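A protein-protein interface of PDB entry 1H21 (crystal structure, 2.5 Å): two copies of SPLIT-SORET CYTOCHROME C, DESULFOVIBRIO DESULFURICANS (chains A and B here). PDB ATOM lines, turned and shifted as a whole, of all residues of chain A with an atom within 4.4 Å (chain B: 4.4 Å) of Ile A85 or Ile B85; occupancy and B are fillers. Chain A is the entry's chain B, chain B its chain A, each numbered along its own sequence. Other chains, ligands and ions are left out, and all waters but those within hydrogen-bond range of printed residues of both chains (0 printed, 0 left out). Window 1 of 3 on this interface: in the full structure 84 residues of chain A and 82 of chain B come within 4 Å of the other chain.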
ATOM      1  N   GLY A  78     -27.894  -4.685  11.887  1.00  0.00           N
ATOM      2  CA  GLY A  78     -27.879  -5.252  13.227  1.00  0.00           C
ATOM      3  C   GLY A  78     -29.086  -6.116  13.483  1.00  0.00           C
ATOM      4  O   GLY A  78     -29.622  -6.151  14.586  1.00  0.00           O
ATOM      5  N   ILE A  79     -29.469  -6.846  12.446  1.00  0.00           N
ATOM      6  CA  ILE A  79     -30.627  -7.746  12.422  1.00  0.00           C
ATOM      7  C   ILE A  79     -31.953  -7.006  12.251  1.00  0.00           C
ATOM      8  O   ILE A  79     -32.564  -6.523  13.216  1.00  0.00           O
ATOM      9  CB  ILE A  79     -30.743  -8.667  13.643  1.00  0.00           C
ATOM     10  CG1 ILE A  79     -29.447  -9.441  13.878  1.00  0.00           C
ATOM     11  CG2 ILE A  79     -31.913  -9.642  13.410  1.00  0.00           C
ATOM     12  CD1 ILE A  79     -29.533 -10.450  15.032  1.00  0.00           C
ATOM     13  N   THR A  84     -28.247  -4.655  16.769  1.00  0.00           N
ATOM     14  CA  THR A  84     -27.508  -5.525  17.649  1.00  0.00           C
ATOM     15  C   THR A  84     -26.124  -5.841  17.044  1.00  0.00           C
ATOM     16  O   THR A  84     -25.441  -4.913  16.602  1.00  0.00           O
ATOM     17  CB  THR A  84     -28.338  -6.774  17.965  1.00  0.00           C
ATOM     18  OG1 THR A  84     -28.445  -7.596  16.801  1.00  0.00           O
ATOM     19  CG2 THR A  84     -29.735  -6.353  18.401  1.00  0.00           C
ATOM     20  N   ILE A  85     -25.698  -7.107  17.013  1.00  0.00           N
ATOM     21  CA  ILE A  85     -24.380  -7.438  16.464  1.00  0.00           C
ATOM     22  C   ILE A  85     -24.227  -6.845  15.063  1.00  0.00           C
ATOM     23  O   ILE A  85     -25.209  -6.751  14.330  1.00  0.00           O
ATOM     24  CB  ILE A  85     -24.161  -8.966  16.443  1.00  0.00           C
ATOM     25  CG1 ILE A  85     -22.780  -9.305  15.881  1.00  0.00           C
ATOM     26  CG2 ILE A  85     -25.276  -9.653  15.677  1.00  0.00           C
ATOM     27  CD1 ILE A  85     -21.628  -9.087  16.843  1.00  0.00           C
ATOM     28  N   CYS A  86     -23.038  -6.340  14.728  1.00  0.00           N
ATOM     29  CA  CYS A  86     -22.835  -5.783  13.391  1.00  0.00           C
ATOM     30  C   CYS A  86     -22.843  -6.933  12.407  1.00  0.00           C
ATOM     31  O   CYS A  86     -22.172  -7.951  12.608  1.00  0.00           O
ATOM     32  CB  CYS A  86     -21.552  -4.950  13.298  1.00  0.00           C
ATOM     33  SG  CYS A  86     -21.907  -3.148  13.286  1.00  0.00           S
ATOM     34  N   GLY A  87     -23.652  -6.769  11.367  1.00  0.00           N
ATOM     35  CA  GLY A  87     -23.834  -7.779  10.341  1.00  0.00           C
ATOM     36  C   GLY A  87     -22.567  -8.324   9.744  1.00  0.00           C
ATOM     37  O   GLY A  87     -22.463  -9.536   9.492  1.00  0.00           O
ATOM     38  N   LEU A  89     -19.682  -8.451  11.215  1.00  0.00           N
ATOM     39  CA  LEU A  89     -19.011  -9.293  12.199  1.00  0.00           C
ATOM     40  C   LEU A  89     -19.630 -10.658  12.290  1.00  0.00           C
ATOM     41  O   LEU A  89     -18.912 -11.662  12.328  1.00  0.00           O
ATOM     42  CB  LEU A  89     -18.999  -8.669  13.582  1.00  0.00           C
ATOM     43  CG  LEU A  89     -18.237  -7.362  13.666  1.00  0.00           C
ATOM     44  CD1 LEU A  89     -18.271  -6.821  15.081  1.00  0.00           C
ATOM     45  CD2 LEU A  89     -16.820  -7.600  13.198  1.00  0.00           C
ATOM     46  N   TYR A  90     -20.953 -10.706  12.381  1.00  0.00           N
ATOM     47  CA  TYR A  90     -21.618 -11.995  12.462  1.00  0.00           C
ATOM     48  C   TYR A  90     -21.405 -12.796  11.183  1.00  0.00           C
ATOM     49  O   TYR A  90     -21.088 -13.987  11.238  1.00  0.00           O
ATOM     50  CB  TYR A  90     -23.116 -11.879  12.741  1.00  0.00           C
ATOM     51  CG  TYR A  90     -23.713 -13.237  12.730  1.00  0.00           C
ATOM     52  CD1 TYR A  90     -23.570 -14.084  13.817  1.00  0.00           C
ATOM     53  CD2 TYR A  90     -24.316 -13.734  11.586  1.00  0.00           C
ATOM     54  CE1 TYR A  90     -23.983 -15.393  13.753  1.00  0.00           C
ATOM     55  CE2 TYR A  90     -24.721 -15.043  11.516  1.00  0.00           C
ATOM     56  CZ  TYR A  90     -24.571 -15.862  12.605  1.00  0.00           C
ATOM     57  OH  TYR A  90     -25.045 -17.146  12.549  1.00  0.00           O
ATOM     58  N   PHE A 113     -13.531  -9.818  16.966  1.00  0.00           N
ATOM     59  CA  PHE A 113     -14.340  -8.886  17.722  1.00  0.00           C
ATOM     60  C   PHE A 113     -13.499  -7.841  18.478  1.00  0.00           C
ATOM     61  O   PHE A 113     -13.775  -6.644  18.397  1.00  0.00           O
ATOM     62  CB  PHE A 113     -15.298  -9.666  18.635  1.00  0.00           C
ATOM     63  CG  PHE A 113     -16.481 -10.297  17.900  1.00  0.00           C
ATOM     64  CD1 PHE A 113     -16.451 -10.482  16.523  1.00  0.00           C
ATOM     65  CD2 PHE A 113     -17.618 -10.690  18.591  1.00  0.00           C
ATOM     66  CE1 PHE A 113     -17.530 -11.042  15.850  1.00  0.00           C
ATOM     67  CE2 PHE A 113     -18.694 -11.251  17.928  1.00  0.00           C
ATOM     68  CZ  PHE A 113     -18.651 -11.425  16.557  1.00  0.00           C
ATOM     69  N   VAL A 145     -19.059  -4.052  19.428  1.00  0.00           N
ATOM     70  CA  VAL A 145     -19.352  -4.918  18.281  1.00  0.00           C
ATOM     71  C   VAL A 145     -20.844  -4.792  17.951  1.00  0.00           C
ATOM     72  O   VAL A 145     -21.370  -5.530  17.113  1.00  0.00           O
ATOM     73  CB  VAL A 145     -19.001  -6.405  18.522  1.00  0.00           C
ATOM     74  CG1 VAL A 145     -17.525  -6.569  18.733  1.00  0.00           C
ATOM     75  CG2 VAL A 145     -19.778  -6.940  19.695  1.00  0.00           C
ATOM     76  N   LEU A 146     -21.512  -3.847  18.614  1.00  0.00           N
ATOM     77  CA  LEU A 146     -22.929  -3.593  18.403  1.00  0.00           C
ATOM     78  C   LEU A 146     -23.149  -2.455  17.428  1.00  0.00           C
ATOM     79  O   LEU A 146     -22.782  -1.318  17.694  1.00  0.00           O
ATOM     80  CB  LEU A 146     -23.622  -3.260  19.725  1.00  0.00           C
ATOM     81  CG  LEU A 146     -23.605  -4.282  20.863  1.00  0.00           C
ATOM     82  CD1 LEU A 146     -24.560  -3.797  21.939  1.00  0.00           C
ATOM     83  CD2 LEU A 146     -24.026  -5.671  20.377  1.00  0.00           C
ATOM     84  N   CYS A 147     -23.818  -2.758  16.329  1.00  0.00           N
ATOM     85  CA  CYS A 147     -24.118  -1.779  15.295  1.00  0.00           C
ATOM     86  C   CYS A 147     -24.732  -0.456  15.808  1.00  0.00           C
ATOM     87  O   CYS A 147     -24.430   0.610  15.273  1.00  0.00           O
ATOM     88  CB  CYS A 147     -24.990  -2.436  14.213  1.00  0.00           C
ATOM     89  SG  CYS A 147     -25.874  -1.311  13.111  1.00  0.00           S
ATOM     90  N   GLY B  78     -24.528 -15.528  22.713  1.00  0.00           N
ATOM     91  CA  GLY B  78     -24.522 -14.237  22.057  1.00  0.00           C
ATOM     92  C   GLY B  78     -23.319 -14.119  21.149  1.00  0.00           C
ATOM     93  O   GLY B  78     -22.832 -13.026  20.923  1.00  0.00           O
ATOM     94  N   ILE B  79     -22.901 -15.245  20.573  1.00  0.00           N
ATOM     95  CA  ILE B  79     -21.740 -15.367  19.668  1.00  0.00           C
ATOM     96  C   ILE B  79     -20.429 -15.514  20.478  1.00  0.00           C
ATOM     97  O   ILE B  79     -19.816 -14.538  20.912  1.00  0.00           O
ATOM     98  CB  ILE B  79     -21.663 -14.201  18.615  1.00  0.00           C
ATOM     99  CG1 ILE B  79     -22.975 -14.079  17.838  1.00  0.00           C
ATOM    100  CG2 ILE B  79     -20.553 -14.444  17.627  1.00  0.00           C
ATOM    101  CD1 ILE B  79     -23.098 -12.769  17.042  1.00  0.00           C
ATOM    102  N   THR B  84     -24.021 -10.735  22.853  1.00  0.00           N
ATOM    103  CA  THR B  84     -24.750  -9.802  21.994  1.00  0.00           C
ATOM    104  C   THR B  84     -26.185 -10.330  21.777  1.00  0.00           C
ATOM    105  O   THR B  84     -26.864 -10.680  22.741  1.00  0.00           O
ATOM    106  CB  THR B  84     -23.993  -9.518  20.637  1.00  0.00           C
ATOM    107  OG1 THR B  84     -23.940 -10.701  19.816  1.00  0.00           O
ATOM    108  CG2 THR B  84     -22.552  -9.020  20.914  1.00  0.00           C
ATOM    109  N   ILE B  85     -26.639 -10.406  20.532  1.00  0.00           N
ATOM    110  CA  ILE B  85     -27.975 -10.891  20.232  1.00  0.00           C
ATOM    111  C   ILE B  85     -28.201 -12.274  20.853  1.00  0.00           C
ATOM    112  O   ILE B  85     -27.309 -13.130  20.797  1.00  0.00           O
ATOM    113  CB  ILE B  85     -28.175 -10.968  18.691  1.00  0.00           C
ATOM    114  CG1 ILE B  85     -29.571 -11.495  18.343  1.00  0.00           C
ATOM    115  CG2 ILE B  85     -27.132 -11.863  18.083  1.00  0.00           C
ATOM    116  CD1 ILE B  85     -30.716 -10.651  18.852  1.00  0.00           C
ATOM    117  N   CYS B  86     -29.353 -12.484  21.492  1.00  0.00           N
ATOM    118  CA  CYS B  86     -29.637 -13.802  22.049  1.00  0.00           C
ATOM    119  C   CYS B  86     -29.743 -14.823  20.919  1.00  0.00           C
ATOM    120  O   CYS B  86     -30.506 -14.643  19.972  1.00  0.00           O
ATOM    121  CB  CYS B  86     -30.878 -13.775  22.933  1.00  0.00           C
ATOM    122  SG  CYS B  86     -30.393 -13.947  24.691  1.00  0.00           S
ATOM    123  N   GLY B  87     -28.885 -15.834  20.976  1.00  0.00           N
ATOM    124  CA  GLY B  87     -28.831 -16.856  19.945  1.00  0.00           C
ATOM    125  C   GLY B  87     -30.148 -17.456  19.487  1.00  0.00           C
ATOM    126  O   GLY B  87     -30.345 -17.737  18.300  1.00  0.00           O
ATOM    127  N   LEU B  89     -32.958 -16.036  19.434  1.00  0.00           N
ATOM    128  CA  LEU B  89     -33.620 -15.023  18.623  1.00  0.00           C
ATOM    129  C   LEU B  89     -33.062 -14.978  17.207  1.00  0.00           C
ATOM    130  O   LEU B  89     -33.820 -14.903  16.229  1.00  0.00           O
ATOM    131  CB  LEU B  89     -33.532 -13.648  19.282  1.00  0.00           C
ATOM    132  CG  LEU B  89     -34.315 -13.373  20.568  1.00  0.00           C
ATOM    133  CD1 LEU B  89     -34.183 -11.897  20.850  1.00  0.00           C
ATOM    134  CD2 LEU B  89     -35.771 -13.689  20.418  1.00  0.00           C
ATOM    135  N   TYR B  90     -31.742 -15.033  17.081  1.00  0.00           N
ATOM    136  CA  TYR B  90     -31.154 -15.013  15.746  1.00  0.00           C
ATOM    137  C   TYR B  90     -31.524 -16.285  14.976  1.00  0.00           C
ATOM    138  O   TYR B  90     -31.973 -16.228  13.830  1.00  0.00           O
ATOM    139  CB  TYR B  90     -29.633 -14.874  15.777  1.00  0.00           C
ATOM    140  CG  TYR B  90     -29.123 -14.855  14.378  1.00  0.00           C
ATOM    141  CD1 TYR B  90     -29.339 -13.742  13.560  1.00  0.00           C
ATOM    142  CD2 TYR B  90     -28.524 -15.983  13.818  1.00  0.00           C
ATOM    143  CE1 TYR B  90     -28.979 -13.758  12.230  1.00  0.00           C
ATOM    144  CE2 TYR B  90     -28.154 -16.005  12.459  1.00  0.00           C
ATOM    145  CZ  TYR B  90     -28.388 -14.889  11.684  1.00  0.00           C
ATOM    146  OH  TYR B  90     -28.025 -14.896  10.373  1.00  0.00           O
ATOM    147  N   PHE B 113     -39.028  -9.946  18.264  1.00  0.00           N
ATOM    148  CA  PHE B 113     -38.166  -9.172  19.163  1.00  0.00           C
ATOM    149  C   PHE B 113     -38.901  -8.335  20.235  1.00  0.00           C
ATOM    150  O   PHE B 113     -38.500  -8.355  21.397  1.00  0.00           O
ATOM    151  CB  PHE B 113     -37.191  -8.300  18.359  1.00  0.00           C
ATOM    152  CG  PHE B 113     -36.065  -9.072  17.705  1.00  0.00           C
ATOM    153  CD1 PHE B 113     -36.129 -10.460  17.560  1.00  0.00           C
ATOM    154  CD2 PHE B 113     -34.948  -8.409  17.223  1.00  0.00           C
ATOM    155  CE1 PHE B 113     -35.101 -11.172  16.948  1.00  0.00           C
ATOM    156  CE2 PHE B 113     -33.912  -9.113  16.608  1.00  0.00           C
ATOM    157  CZ  PHE B 113     -33.994 -10.497  16.471  1.00  0.00           C
ATOM    158  N   VAL B 145     -33.100  -7.624  23.886  1.00  0.00           N
ATOM    159  CA  VAL B 145     -32.909  -8.692  22.941  1.00  0.00           C
ATOM    160  C   VAL B 145     -31.446  -9.169  23.050  1.00  0.00           C
ATOM    161  O   VAL B 145     -31.076 -10.239  22.547  1.00  0.00           O
ATOM    162  CB  VAL B 145     -33.279  -8.101  21.568  1.00  0.00           C
ATOM    163  CG1 VAL B 145     -32.390  -8.586  20.491  1.00  0.00           C
ATOM    164  CG2 VAL B 145     -34.741  -8.389  21.267  1.00  0.00           C
ATOM    165  N   LEU B 146     -30.656  -8.412  23.811  1.00  0.00           N
ATOM    166  CA  LEU B 146     -29.245  -8.695  24.020  1.00  0.00           C
ATOM    167  C   LEU B 146     -29.036  -9.660  25.167  1.00  0.00           C
ATOM    168  O   LEU B 146     -29.542  -9.429  26.256  1.00  0.00           O
ATOM    169  CB  LEU B 146     -28.497  -7.391  24.293  1.00  0.00           C
ATOM    170  CG  LEU B 146     -28.473  -6.382  23.140  1.00  0.00           C
ATOM    171  CD1 LEU B 146     -27.644  -5.172  23.524  1.00  0.00           C
ATOM    172  CD2 LEU B 146     -27.927  -7.061  21.869  1.00  0.00           C
ATOM    173  N   CYS B 147     -28.295 -10.733  24.905  1.00  0.00           N
ATOM    174  CA  CYS B 147     -27.956 -11.782  25.871  1.00  0.00           C
ATOM    175  C   CYS B 147     -27.319 -11.278  27.174  1.00  0.00           C
ATOM    176  O   CYS B 147     -27.636 -11.765  28.260  1.00  0.00           O
ATOM    177  CB  CYS B 147     -26.978 -12.741  25.206  1.00  0.00           C
ATOM    178  SG  CYS B 147     -27.289 -14.457  25.441  1.00  0.00           S
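OG1 of Thr B84 sits at hydrogen-bond distance from O of Gly B78, at 2.8 Å.
O of Thr B84 is in hydrogen-bond range of N of Cys B147 (2.6 Å).
The side-chain hydroxyl of Thr A84 lies within hydrogen-bond range of the backbone carbonyl oxygen of Gly A78, 2.9 Å away.
The backbone carbonyl oxygen of Thr A84 sits at hydrogen-bond distance from the backbone NH of Cys A147.
N of Cys A86 lies within hydrogen-bond range of O of Val A145 (3.0 Å).
Ile B85 touches Ile A79 (CG1 to CD1, 3.5 Å).
Tyr B90 touches Ile A79 (CD1 to CD1, 3.6 Å).
Ile A79 touches Phe B113 (CG2 to CZ, 3.8 Å).
CB of Ile B85 touches OG1 of Thr A84, at 3.9 Å.
CB of Thr A84 touches CD2 of Leu B146, at 3.9 Å.
Ile B79 touches Ile A85 (CD1 to CG1, 3.7 Å).
Ile A85 touches Ile B85 (CG2 to CG2, 3.8 Å).
CD1 of Ile B79 touches CD1 of Tyr A90, 3.5 Å away.
Ile B79 touches Phe A113.
CD1 of Leu B146 touches CD1 of Leu A146 (3.7 Å).
Printed residues of chain B within 4 Å of Ile A79: Ile B85, Tyr B90 and Phe B113.
Printed residues of chain B within 4 Å of Thr A84: Ile B85 and Leu B146.
Ile A85 touches three residues of chain B.
Printed residues of chain B within 4 Å of Tyr A90: Ile B79 (3.5 Å) and Tyr B90 (3.3 Å).
Of the printed residues of chain A, Ile B79 touches Ile A85, Tyr A90 and Phe A113.
Ile B85 touches just these residues of chain A: Ile A79, Thr A84 and Ile A85.
Printed residues of chain A within 4 Å of Tyr B90: Ile A79 (3.6 Å) and Tyr A90 (3.3 Å).
Hydrophobic or aromatic side chains of chain A within 4 Å of the printed part of chain B: Ile A79, Ile A85, Tyr A90, Phe A113, Val A145 and Leu A146.
Along chain A the printed residues that touch a printed residue of chain B span positions 79 to 146.
Printed residues of chain B that touch a printed residue of chain A: Ile B79, Thr B84, Ile B85, Tyr B90, Phe B113 and Leu B146.
Along chain B the printed residues that touch a printed residue of chain A span positions 79 to 146.
Among the printed residues, no Asp or Glu carboxylate lies within 4 Å of a Lys or Arg side-chain nitrogen of the other chain.
Thr A84 touches Ile B85, and with the chains exchanged Ile A85 touches Thr B84.
Thr A84 touches Leu B146, and with the chains exchanged Leu A146 touches Thr B84.
Ile A85 touches its own counterpart, Ile B85.
Tyr A90 touches its own counterpart, Tyr B90.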
